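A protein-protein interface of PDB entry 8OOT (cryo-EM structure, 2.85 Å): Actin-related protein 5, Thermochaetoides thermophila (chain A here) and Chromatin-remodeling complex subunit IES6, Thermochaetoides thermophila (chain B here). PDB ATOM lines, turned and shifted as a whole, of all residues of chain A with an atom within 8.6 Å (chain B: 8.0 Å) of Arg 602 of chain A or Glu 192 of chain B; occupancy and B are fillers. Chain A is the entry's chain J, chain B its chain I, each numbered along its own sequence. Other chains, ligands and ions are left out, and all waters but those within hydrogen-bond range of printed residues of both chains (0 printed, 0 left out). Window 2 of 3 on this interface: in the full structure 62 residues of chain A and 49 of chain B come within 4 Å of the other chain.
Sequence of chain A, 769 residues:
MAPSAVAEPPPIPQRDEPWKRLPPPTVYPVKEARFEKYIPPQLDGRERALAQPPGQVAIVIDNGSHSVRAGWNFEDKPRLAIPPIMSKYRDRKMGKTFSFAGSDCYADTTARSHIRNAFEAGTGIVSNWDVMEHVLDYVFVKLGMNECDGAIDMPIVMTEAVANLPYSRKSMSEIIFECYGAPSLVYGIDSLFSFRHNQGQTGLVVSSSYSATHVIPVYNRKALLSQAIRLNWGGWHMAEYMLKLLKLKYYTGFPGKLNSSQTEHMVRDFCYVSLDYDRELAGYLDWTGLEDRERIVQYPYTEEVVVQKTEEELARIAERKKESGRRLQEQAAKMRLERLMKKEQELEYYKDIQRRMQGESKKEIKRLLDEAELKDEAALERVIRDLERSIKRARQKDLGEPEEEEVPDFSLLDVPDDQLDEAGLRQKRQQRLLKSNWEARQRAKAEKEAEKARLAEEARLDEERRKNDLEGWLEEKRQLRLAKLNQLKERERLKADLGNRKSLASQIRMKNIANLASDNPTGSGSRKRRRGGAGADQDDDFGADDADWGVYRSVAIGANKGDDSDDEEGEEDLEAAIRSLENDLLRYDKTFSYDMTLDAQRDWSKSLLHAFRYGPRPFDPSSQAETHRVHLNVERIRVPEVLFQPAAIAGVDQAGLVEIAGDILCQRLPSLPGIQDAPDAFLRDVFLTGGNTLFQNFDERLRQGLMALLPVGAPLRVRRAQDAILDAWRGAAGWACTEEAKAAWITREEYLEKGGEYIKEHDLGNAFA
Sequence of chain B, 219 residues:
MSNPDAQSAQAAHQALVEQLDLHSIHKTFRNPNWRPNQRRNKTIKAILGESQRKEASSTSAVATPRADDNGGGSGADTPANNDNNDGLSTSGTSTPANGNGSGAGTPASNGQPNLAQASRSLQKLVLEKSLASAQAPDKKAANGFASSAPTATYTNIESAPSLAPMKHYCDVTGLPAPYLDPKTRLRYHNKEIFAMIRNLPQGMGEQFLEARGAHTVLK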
ATOM      1  N   TRP A 287      27.550   6.459   5.681  1.00  0.00           N
ATOM      2  CA  TRP A 287      26.950   6.752   6.980  1.00  0.00           C
ATOM      3  C   TRP A 287      27.674   7.871   7.715  1.00  0.00           C
ATOM      4  O   TRP A 287      27.039   8.652   8.431  1.00  0.00           O
ATOM      5  CB  TRP A 287      26.925   5.487   7.836  1.00  0.00           C
ATOM      6  CG  TRP A 287      25.738   4.625   7.573  1.00  0.00           C
ATOM      7  CD1 TRP A 287      25.619   3.658   6.619  1.00  0.00           C
ATOM      8  CD2 TRP A 287      24.491   4.652   8.274  1.00  0.00           C
ATOM      9  NE1 TRP A 287      24.374   3.081   6.683  1.00  0.00           N
ATOM     10  CE2 TRP A 287      23.662   3.676   7.692  1.00  0.00           C
ATOM     11  CE3 TRP A 287      23.996   5.408   9.339  1.00  0.00           C
ATOM     12  CZ2 TRP A 287      22.368   3.436   8.138  1.00  0.00           C
ATOM     13  CZ3 TRP A 287      22.712   5.168   9.782  1.00  0.00           C
ATOM     14  CH2 TRP A 287      21.912   4.191   9.182  1.00  0.00           C
ATOM     15  N   GLN A 601      22.652  -9.288  14.383  1.00  0.00           N
ATOM     16  CA  GLN A 601      23.674  -8.249  14.412  1.00  0.00           C
ATOM     17  C   GLN A 601      23.793  -7.562  13.056  1.00  0.00           C
ATOM     18  O   GLN A 601      24.694  -6.758  12.828  1.00  0.00           O
ATOM     19  CB  GLN A 601      25.020  -8.841  14.840  1.00  0.00           C
ATOM     20  CG  GLN A 601      25.611  -9.838  13.858  1.00  0.00           C
ATOM     21  CD  GLN A 601      26.979 -10.334  14.287  1.00  0.00           C
ATOM     22  OE1 GLN A 601      27.390 -10.140  15.432  1.00  0.00           O
ATOM     23  NE2 GLN A 601      27.688 -10.982  13.371  1.00  0.00           N
ATOM     24  N   ARG A 602      22.868  -7.892  12.160  1.00  0.00           N
ATOM     25  CA  ARG A 602      22.588  -7.102  10.968  1.00  0.00           C
ATOM     26  C   ARG A 602      21.247  -6.412  11.172  1.00  0.00           C
ATOM     27  O   ARG A 602      20.225  -7.080  11.359  1.00  0.00           O
ATOM     28  CB  ARG A 602      22.563  -7.985   9.720  1.00  0.00           C
ATOM     29  CG  ARG A 602      22.065  -7.285   8.468  1.00  0.00           C
ATOM     30  CD  ARG A 602      22.843  -6.009   8.195  1.00  0.00           C
ATOM     31  NE  ARG A 602      22.545  -5.459   6.877  1.00  0.00           N
ATOM     32  CZ  ARG A 602      23.247  -5.718   5.782  1.00  0.00           C
ATOM     33  NH1 ARG A 602      24.270  -6.556   5.800  1.00  0.00           N
ATOM     34  NH2 ARG A 602      22.901  -5.136   4.637  1.00  0.00           N
ATOM     35  N   ASP A 603      21.248  -5.082  11.130  1.00  0.00           N
ATOM     36  CA  ASP A 603      20.037  -4.319  11.399  1.00  0.00           C
ATOM     37  C   ASP A 603      20.038  -3.045  10.559  1.00  0.00           C
ATOM     38  O   ASP A 603      20.842  -2.886   9.636  1.00  0.00           O
ATOM     39  CB  ASP A 603      19.903  -4.052  12.907  1.00  0.00           C
ATOM     40  CG  ASP A 603      20.955  -3.083  13.450  1.00  0.00           C
ATOM     41  OD1 ASP A 603      21.689  -2.442  12.668  1.00  0.00           O
ATOM     42  OD2 ASP A 603      21.046  -2.962  14.689  1.00  0.00           O
ATOM     43  N   TRP A 604      19.105  -2.145  10.886  1.00  0.00           N
ATOM     44  CA  TRP A 604      18.947  -0.884  10.165  1.00  0.00           C
ATOM     45  C   TRP A 604      20.247  -0.091  10.090  1.00  0.00           C
ATOM     46  O   TRP A 604      20.544   0.529   9.063  1.00  0.00           O
ATOM     47  CB  TRP A 604      17.838  -0.054  10.815  1.00  0.00           C
ATOM     48  CG  TRP A 604      18.171   0.488  12.171  1.00  0.00           C
ATOM     49  CD1 TRP A 604      17.874  -0.081  13.373  1.00  0.00           C
ATOM     50  CD2 TRP A 604      18.825   1.729  12.465  1.00  0.00           C
ATOM     51  NE1 TRP A 604      18.322   0.717  14.397  1.00  0.00           N
ATOM     52  CE2 TRP A 604      18.907   1.835  13.865  1.00  0.00           C
ATOM     53  CE3 TRP A 604      19.357   2.753  11.679  1.00  0.00           C
ATOM     54  CZ2 TRP A 604      19.499   2.924  14.497  1.00  0.00           C
ATOM     55  CZ3 TRP A 604      19.943   3.834  12.307  1.00  0.00           C
ATOM     56  CH2 TRP A 604      20.010   3.912  13.701  1.00  0.00           C
ATOM     57  N   SER A 605      21.037  -0.101  11.164  1.00  0.00           N
ATOM     58  CA  SER A 605      22.256   0.699  11.203  1.00  0.00           C
ATOM     59  C   SER A 605      23.291   0.246  10.184  1.00  0.00           C
ATOM     60  O   SER A 605      24.204   1.013   9.865  1.00  0.00           O
ATOM     61  CB  SER A 605      22.865   0.664  12.605  1.00  0.00           C
ATOM     62  OG  SER A 605      24.006   1.499  12.684  1.00  0.00           O
ATOM     63  N   LYS A 606      23.180  -0.976   9.671  1.00  0.00           N
ATOM     64  CA  LYS A 606      24.061  -1.453   8.614  1.00  0.00           C
ATOM     65  C   LYS A 606      23.395  -1.465   7.247  1.00  0.00           C
ATOM     66  O   LYS A 606      24.053  -1.794   6.256  1.00  0.00           O
ATOM     67  CB  LYS A 606      24.575  -2.859   8.941  1.00  0.00           C
ATOM     68  CG  LYS A 606      25.515  -2.930  10.131  1.00  0.00           C
ATOM     69  CD  LYS A 606      25.971  -4.360  10.366  1.00  0.00           C
ATOM     70  CE  LYS A 606      26.847  -4.471  11.601  1.00  0.00           C
ATOM     71  NZ  LYS A 606      27.147  -5.891  11.930  1.00  0.00           N
ATOM     72  N   SER A 607      22.113  -1.119   7.166  1.00  0.00           N
ATOM     73  CA  SER A 607      21.413  -1.112   5.892  1.00  0.00           C
ATOM     74  C   SER A 607      21.663   0.186   5.134  1.00  0.00           C
ATOM     75  O   SER A 607      21.874   1.252   5.720  1.00  0.00           O
ATOM     76  CB  SER A 607      19.914  -1.316   6.099  1.00  0.00           C
ATOM     77  OG  SER A 607      19.315  -0.150   6.621  1.00  0.00           O
ATOM     78  N   LEU A 608      21.631   0.077   3.807  1.00  0.00           N
ATOM     79  CA  LEU A 608      21.735   1.228   2.917  1.00  0.00           C
ATOM     80  C   LEU A 608      20.403   1.945   2.744  1.00  0.00           C
ATOM     81  O   LEU A 608      20.355   3.181   2.734  1.00  0.00           O
ATOM     82  CB  LEU A 608      22.265   0.770   1.558  1.00  0.00           C
ATOM     83  CG  LEU A 608      22.354   1.801   0.436  1.00  0.00           C
ATOM     84  CD1 LEU A 608      23.257   2.951   0.840  1.00  0.00           C
ATOM     85  CD2 LEU A 608      22.846   1.147  -0.841  1.00  0.00           C
ATOM     86  N   LEU A 609      19.315   1.187   2.611  1.00  0.00           N
ATOM     87  CA  LEU A 609      18.004   1.772   2.358  1.00  0.00           C
ATOM     88  C   LEU A 609      17.481   2.585   3.534  1.00  0.00           C
ATOM     89  O   LEU A 609      16.711   3.529   3.329  1.00  0.00           O
ATOM     90  CB  LEU A 609      17.008   0.677   1.992  1.00  0.00           C
ATOM     91  CG  LEU A 609      17.222   0.077   0.605  1.00  0.00           C
ATOM     92  CD1 LEU A 609      16.371  -1.163   0.424  1.00  0.00           C
ATOM     93  CD2 LEU A 609      16.901   1.111  -0.455  1.00  0.00           C
ATOM     94  N   HIS A 610      17.872   2.252   4.763  1.00  0.00           N
ATOM     95  CA  HIS A 610      17.549   3.150   5.868  1.00  0.00           C
ATOM     96  C   HIS A 610      18.259   4.488   5.720  1.00  0.00           C
ATOM     97  O   HIS A 610      17.653   5.542   5.940  1.00  0.00           O
ATOM     98  CB  HIS A 610      17.911   2.503   7.200  1.00  0.00           C
ATOM     99  CG  HIS A 610      17.495   3.304   8.391  1.00  0.00           C
ATOM    100  ND1 HIS A 610      16.351   3.033   9.107  1.00  0.00           N
ATOM    101  CD2 HIS A 610      18.070   4.374   8.989  1.00  0.00           C
ATOM    102  CE1 HIS A 610      16.239   3.900  10.098  1.00  0.00           C
ATOM    103  NE2 HIS A 610      17.269   4.725  10.047  1.00  0.00           N
ATOM    104  N   ALA A 611      19.544   4.470   5.364  1.00  0.00           N
ATOM    105  CA  ALA A 611      20.260   5.722   5.141  1.00  0.00           C
ATOM    106  C   ALA A 611      19.626   6.518   4.009  1.00  0.00           C
ATOM    107  O   ALA A 611      19.437   7.734   4.118  1.00  0.00           O
ATOM    108  CB  ALA A 611      21.730   5.437   4.841  1.00  0.00           C
ATOM    109  N   PHE A 612      19.296   5.835   2.913  1.00  0.00           N
ATOM    110  CA  PHE A 612      18.627   6.467   1.781  1.00  0.00           C
ATOM    111  C   PHE A 612      17.309   7.116   2.186  1.00  0.00           C
ATOM    112  O   PHE A 612      17.019   8.248   1.785  1.00  0.00           O
ATOM    113  CB  PHE A 612      18.405   5.416   0.692  1.00  0.00           C
ATOM    114  CG  PHE A 612      17.722   5.932  -0.537  1.00  0.00           C
ATOM    115  CD1 PHE A 612      18.246   7.001  -1.239  1.00  0.00           C
ATOM    116  CD2 PHE A 612      16.578   5.319  -1.016  1.00  0.00           C
ATOM    117  CE1 PHE A 612      17.629   7.464  -2.381  1.00  0.00           C
ATOM    118  CE2 PHE A 612      15.956   5.780  -2.159  1.00  0.00           C
ATOM    119  CZ  PHE A 612      16.484   6.851  -2.843  1.00  0.00           C
ATOM    120  N   ARG A 613      16.497   6.419   2.980  1.00  0.00           N
ATOM    121  CA  ARG A 613      15.162   6.897   3.318  1.00  0.00           C
ATOM    122  C   ARG A 613      15.109   7.723   4.597  1.00  0.00           C
ATOM    123  O   ARG A 613      14.282   8.635   4.698  1.00  0.00           O
ATOM    124  CB  ARG A 613      14.197   5.718   3.426  1.00  0.00           C
ATOM    125  CG  ARG A 613      13.937   5.048   2.097  1.00  0.00           C
ATOM    126  CD  ARG A 613      12.935   3.926   2.224  1.00  0.00           C
ATOM    127  NE  ARG A 613      12.588   3.376   0.922  1.00  0.00           N
ATOM    128  CZ  ARG A 613      12.901   2.153   0.520  1.00  0.00           C
ATOM    129  NH1 ARG A 613      13.376   1.251   1.362  1.00  0.00           N
ATOM    130  NH2 ARG A 613      12.674   1.808  -0.744  1.00  0.00           N
ATOM    131  N   VAL B 172      16.829   2.408  -7.939  1.00  0.00           N
ATOM    132  CA  VAL B 172      16.256   2.663  -6.623  1.00  0.00           C
ATOM    133  C   VAL B 172      16.881   3.894  -5.980  1.00  0.00           C
ATOM    134  O   VAL B 172      16.171   4.801  -5.533  1.00  0.00           O
ATOM    135  CB  VAL B 172      16.400   1.420  -5.727  1.00  0.00           C
ATOM    136  CG1 VAL B 172      15.840   1.702  -4.349  1.00  0.00           C
ATOM    137  CG2 VAL B 172      15.682   0.243  -6.355  1.00  0.00           C
ATOM    138  N   THR B 173      18.211   3.955  -5.917  1.00  0.00           N
ATOM    139  CA  THR B 173      18.887   4.993  -5.150  1.00  0.00           C
ATOM    140  C   THR B 173      19.633   6.010  -6.003  1.00  0.00           C
ATOM    141  O   THR B 173      20.050   7.044  -5.474  1.00  0.00           O
ATOM    142  CB  THR B 173      19.874   4.362  -4.158  1.00  0.00           C
ATOM    143  OG1 THR B 173      20.869   3.626  -4.878  1.00  0.00           O
ATOM    144  CG2 THR B 173      19.150   3.428  -3.209  1.00  0.00           C
ATOM    145  N   TYR B 188      20.689  -1.853 -10.359  1.00  0.00           N
ATOM    146  CA  TYR B 188      20.789  -1.852  -8.909  1.00  0.00           C
ATOM    147  C   TYR B 188      22.240  -1.752  -8.464  1.00  0.00           C
ATOM    148  O   TYR B 188      23.155  -2.245  -9.128  1.00  0.00           O
ATOM    149  CB  TYR B 188      20.093  -3.084  -8.309  1.00  0.00           C
ATOM    150  CG  TYR B 188      20.654  -4.424  -8.714  1.00  0.00           C
ATOM    151  CD1 TYR B 188      20.235  -5.039  -9.885  1.00  0.00           C
ATOM    152  CD2 TYR B 188      21.558  -5.097  -7.909  1.00  0.00           C
ATOM    153  CE1 TYR B 188      20.724  -6.267 -10.262  1.00  0.00           C
ATOM    154  CE2 TYR B 188      22.054  -6.331  -8.276  1.00  0.00           C
ATOM    155  CZ  TYR B 188      21.630  -6.912  -9.452  1.00  0.00           C
ATOM    156  OH  TYR B 188      22.117  -8.141  -9.829  1.00  0.00           O
ATOM    157  N   HIS B 189      22.423  -1.106  -7.312  1.00  0.00           N
ATOM    158  CA  HIS B 189      23.742  -0.808  -6.768  1.00  0.00           C
ATOM    159  C   HIS B 189      24.376  -2.013  -6.087  1.00  0.00           C
ATOM    160  O   HIS B 189      25.570  -2.271  -6.269  1.00  0.00           O
ATOM    161  CB  HIS B 189      23.632   0.359  -5.789  1.00  0.00           C
ATOM    162  CG  HIS B 189      24.931   0.753  -5.162  1.00  0.00           C
ATOM    163  ND1 HIS B 189      25.990   1.252  -5.889  1.00  0.00           N
ATOM    164  CD2 HIS B 189      25.334   0.741  -3.871  1.00  0.00           C
ATOM    165  CE1 HIS B 189      26.993   1.520  -5.074  1.00  0.00           C
ATOM    166  NE2 HIS B 189      26.621   1.220  -3.844  1.00  0.00           N
ATOM    167  N   ASN B 190      23.604  -2.763  -5.306  1.00  0.00           N
ATOM    168  CA  ASN B 190      24.166  -3.845  -4.509  1.00  0.00           C
ATOM    169  C   ASN B 190      23.082  -4.871  -4.214  1.00  0.00           C
ATOM    170  O   ASN B 190      21.907  -4.676  -4.529  1.00  0.00           O
ATOM    171  CB  ASN B 190      24.831  -3.310  -3.231  1.00  0.00           C
ATOM    172  CG  ASN B 190      23.841  -2.758  -2.215  1.00  0.00           C
ATOM    173  OD1 ASN B 190      22.628  -2.856  -2.375  1.00  0.00           O
ATOM    174  ND2 ASN B 190      24.372  -2.171  -1.152  1.00  0.00           N
ATOM    175  N   LYS B 191      23.506  -5.980  -3.604  1.00  0.00           N
ATOM    176  CA  LYS B 191      22.616  -7.103  -3.333  1.00  0.00           C
ATOM    177  C   LYS B 191      21.509  -6.779  -2.338  1.00  0.00           C
ATOM    178  O   LYS B 191      20.474  -7.453  -2.353  1.00  0.00           O
ATOM    179  CB  LYS B 191      23.438  -8.292  -2.833  1.00  0.00           C
ATOM    180  CG  LYS B 191      23.926  -8.157  -1.401  1.00  0.00           C
ATOM    181  CD  LYS B 191      24.970  -9.212  -1.074  1.00  0.00           C
ATOM    182  CE  LYS B 191      24.470 -10.613  -1.394  1.00  0.00           C
ATOM    183  NZ  LYS B 191      23.426 -11.082  -0.444  1.00  0.00           N
ATOM    184  N   GLU B 192      21.693  -5.779  -1.475  1.00  0.00           N
ATOM    185  CA  GLU B 192      20.584  -5.314  -0.647  1.00  0.00           C
ATOM    186  C   GLU B 192      19.455  -4.740  -1.495  1.00  0.00           C
ATOM    187  O   GLU B 192      18.278  -5.026  -1.254  1.00  0.00           O
ATOM    188  CB  GLU B 192      21.071  -4.276   0.361  1.00  0.00           C
ATOM    189  CG  GLU B 192      19.950  -3.653   1.171  1.00  0.00           C
ATOM    190  CD  GLU B 192      20.453  -2.920   2.394  1.00  0.00           C
ATOM    191  OE1 GLU B 192      21.138  -3.550   3.225  1.00  0.00           O
ATOM    192  OE2 GLU B 192      20.158  -1.716   2.528  1.00  0.00           O
ATOM    193  N   ILE B 193      19.798  -3.928  -2.494  1.00  0.00           N
ATOM    194  CA  ILE B 193      18.799  -3.362  -3.393  1.00  0.00           C
ATOM    195  C   ILE B 193      18.235  -4.417  -4.338  1.00  0.00           C
ATOM    196  O   ILE B 193      17.060  -4.358  -4.716  1.00  0.00           O
ATOM    197  CB  ILE B 193      19.415  -2.173  -4.156  1.00  0.00           C
ATOM    198  CG1 ILE B 193      19.601  -0.987  -3.211  1.00  0.00           C
ATOM    199  CG2 ILE B 193      18.558  -1.773  -5.340  1.00  0.00           C
ATOM    200  CD1 ILE B 193      20.623   0.010  -3.684  1.00  0.00           C
ATOM    201  N   PHE B 194      19.040  -5.413  -4.710  1.00  0.00           N
ATOM    202  CA  PHE B 194      18.505  -6.560  -5.436  1.00  0.00           C
ATOM    203  C   PHE B 194      17.443  -7.297  -4.628  1.00  0.00           C
ATOM    204  O   PHE B 194      16.449  -7.774  -5.186  1.00  0.00           O
ATOM    205  CB  PHE B 194      19.640  -7.510  -5.811  1.00  0.00           C
ATOM    206  CG  PHE B 194      19.200  -8.692  -6.620  1.00  0.00           C
ATOM    207  CD1 PHE B 194      19.024  -8.586  -7.986  1.00  0.00           C
ATOM    208  CD2 PHE B 194      18.962  -9.913  -6.014  1.00  0.00           C
ATOM    209  CE1 PHE B 194      18.623  -9.674  -8.732  1.00  0.00           C
ATOM    210  CE2 PHE B 194      18.559 -11.002  -6.755  1.00  0.00           C
ATOM    211  CZ  PHE B 194      18.389 -10.882  -8.115  1.00  0.00           C
ATOM    212  N   ALA B 195      17.644  -7.419  -3.317  1.00  0.00           N
ATOM    213  CA  ALA B 195      16.627  -8.021  -2.460  1.00  0.00           C
ATOM    214  C   ALA B 195      15.327  -7.224  -2.475  1.00  0.00           C
ATOM    215  O   ALA B 195      14.238  -7.792  -2.607  1.00  0.00           O
ATOM    216  CB  ALA B 195      17.160  -8.146  -1.033  1.00  0.00           C
ATOM    217  N   MET B 196      15.425  -5.902  -2.335  1.00  0.00           N
ATOM    218  CA  MET B 196      14.274  -5.018  -2.509  1.00  0.00           C
ATOM    219  C   MET B 196      13.586  -5.204  -3.859  1.00  0.00           C
ATOM    220  O   MET B 196      12.370  -5.413  -3.924  1.00  0.00           O
ATOM    221  CB  MET B 196      14.714  -3.564  -2.337  1.00  0.00           C
ATOM    222  CG  MET B 196      13.792  -2.556  -2.999  1.00  0.00           C
ATOM    223  SD  MET B 196      13.701  -1.005  -2.093  1.00  0.00           S
ATOM    224  CE  MET B 196      12.739  -1.510  -0.670  1.00  0.00           C
ATOM    225  N   ILE B 197      14.352  -5.117  -4.947  1.00  0.00           N
ATOM    226  CA  ILE B 197      13.779  -5.089  -6.292  1.00  0.00           C
ATOM    227  C   ILE B 197      12.910  -6.311  -6.570  1.00  0.00           C
ATOM    228  O   ILE B 197      11.823  -6.193  -7.150  1.00  0.00           O
ATOM    229  CB  ILE B 197      14.901  -4.942  -7.335  1.00  0.00           C
ATOM    230  CG1 ILE B 197      15.332  -3.481  -7.429  1.00  0.00           C
ATOM    231  CG2 ILE B 197      14.456  -5.453  -8.686  1.00  0.00           C
ATOM    232  CD1 ILE B 197      16.593  -3.281  -8.213  1.00  0.00           C
ATOM    233  N   ARG B 198      13.353  -7.494  -6.160  1.00  0.00           N
ATOM    234  CA  ARG B 198      12.538  -8.684  -6.371  1.00  0.00           C
ATOM    235  C   ARG B 198      11.470  -8.893  -5.304  1.00  0.00           C
ATOM    236  O   ARG B 198      10.666  -9.822  -5.435  1.00  0.00           O
ATOM    237  CB  ARG B 198      13.435  -9.914  -6.499  1.00  0.00           C
ATOM    238  CG  ARG B 198      14.232  -9.882  -7.793  1.00  0.00           C
ATOM    239  CD  ARG B 198      14.735 -11.243  -8.212  1.00  0.00           C
ATOM    240  NE  ARG B 198      15.391 -11.174  -9.510  1.00  0.00           N
ATOM    241  CZ  ARG B 198      15.861 -12.222 -10.172  1.00  0.00           C
ATOM    242  NH1 ARG B 198      15.625 -13.459  -9.765  1.00  0.00           N
ATOM    243  NH2 ARG B 198      16.538 -12.027 -11.300  1.00  0.00           N
ATOM    244  N   ASN B 199      11.438  -8.068  -4.262  1.00  0.00           N
ATOM    245  CA  ASN B 199      10.355  -8.068  -3.289  1.00  0.00           C
ATOM    246  C   ASN B 199       9.353  -6.942  -3.526  1.00  0.00           C
ATOM    247  O   ASN B 199       8.481  -6.715  -2.682  1.00  0.00           O
ATOM    248  CB  ASN B 199      10.918  -7.975  -1.871  1.00  0.00           C
ATOM    249  CG  ASN B 199      11.749  -9.182  -1.497  1.00  0.00           C
ATOM    250  OD1 ASN B 199      11.742 -10.194  -2.197  1.00  0.00           O
ATOM    251  ND2 ASN B 199      12.473  -9.081  -0.390  1.00  0.00           N
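Of the 14 printed residues of chain B, 7 touch a printed residue of chain A. Printed residues of chain B that touch a printed residue of chain A: Val 172, Thr 173, His 189, Asn 190, Glu 192, Ile 193 and Met 196. Hydrophobic or aromatic side chains of chain B within 4 Å of the printed part of chain A: His 189, Ile 193 and Met 196. Of the 14 printed residues of chain A, 6 touch a printed residue of chain B. Printed residues of chain A that touch a printed residue of chain B: Arg 602, Ser 607, Leu 608, Leu 609, Phe 612 and Arg 613. Hydrophobic or aromatic side chains of chain A within 4 Å of the printed part of chain B: Leu 608, Leu 609 and Phe 612. Among the printed residues, 11 pairs touch across the chains. Among the printed residues, Asp or Glu carboxylates within 4 Å of a Lys or Arg side-chain nitrogen of the other chain: Arg 602 of chain A with Glu 192 of chain B.
Glu 192 of chain B touches Ser 607 of chain A (OE2 to C, 3.6 Å). CD2 of Leu 608 of chain A touches CD2 of His 189 of chain B, 3.9 Å away. ND2 of Asn 190 of chain B touches CD2 of Leu 608 of chain A, 3.7 Å away. Ile 193 of chain B touches Leu 608 of chain A. CD1 of Leu 609 of chain A touches SD of Met 196 of chain B, 3.7 Å away. Phe 612 of chain A touches Val 172 of chain B. Phe 612 of chain A touches Thr 173 of chain B (CZ to CA, 3.8 Å).
The side-chain sulfur (SD) of Met 196 of chain B sits at hydrogen-bond distance from the guanidinium group (NH2) of Arg 613 of chain A, 3.3 Å away. The guanidinium group (NH2) of Arg 602 of chain A is in salt-bridge range of the side-chain carboxylate (OE1) of Glu 192 of chain B, 2.8 Å away. OE2 of Glu 192 of chain B is in hydrogen-bond range of N of Leu 609 of chain A (3.0 Å). OE2 of Glu 192 of chain B sits at hydrogen-bond distance from N of Leu 608 of chain A (2.6 Å).
Arg 602 of chain A touches just one residue of chain B: Glu 192 (2.8 Å). Of chain A, only Arg 602 (2.8 Å), Ser 607 (3.6 Å), Leu 608 (2.6 Å) and Leu 609 (3.0 Å) come within 4 Å of Glu 192 of chain B. Of the printed residues of chain B, Phe 612 of chain A touches Val 172 (3.4 Å) and Thr 173 (3.8 Å). Of the printed residues of chain A, His 189 of chain B touches Leu 608. Of the printed residues of chain B, Leu 608 of chain A touches His 189, Asn 190, Glu 192 and Ile 193. Printed residues of chain A within 4 Å of Asn 190 of chain B: Leu 608 (3.7 Å). Of the printed residues of chain A, Met 196 of chain B touches Leu 609 (3.7 Å) and Arg 613 (3.3 Å). Trp 287 of chain A touches none of the printed residues of chain B. Ser 605 of chain A touches none of the printed residues of chain B. The nearest residue of chain A that does not touch Glu 192 of chain B is Lys 606 of chain A (4.6 Å). The nearest printed residue of chain B that does not touch Arg 613 of chain A is Val 172 of chain B (4.8 Å).
OD1 of Asn 190 of chain B lies within hydrogen-bond range of N of Glu 192 of chain B, 3.2 Å away. The side-chain hydroxyl (OG) of Ser 607 of chain A lies within hydrogen-bond range of the backbone carbonyl oxygen (O) of Trp 604 of chain A (2.8 Å). The side-chain amide oxygen (OD1) of Asn 190 of chain B is in hydrogen-bond range of the backbone NH (N) of Ile 193 of chain B (3.0 Å). The backbone carbonyl oxygen (O) of Ser 607 of chain A lies within hydrogen-bond range of the indole nitrogen (NE1) of Trp 287 of chain A. The side-chain hydroxyl of Ser 607 of chain A lies close to the backbone NH of His 610 of chain A.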
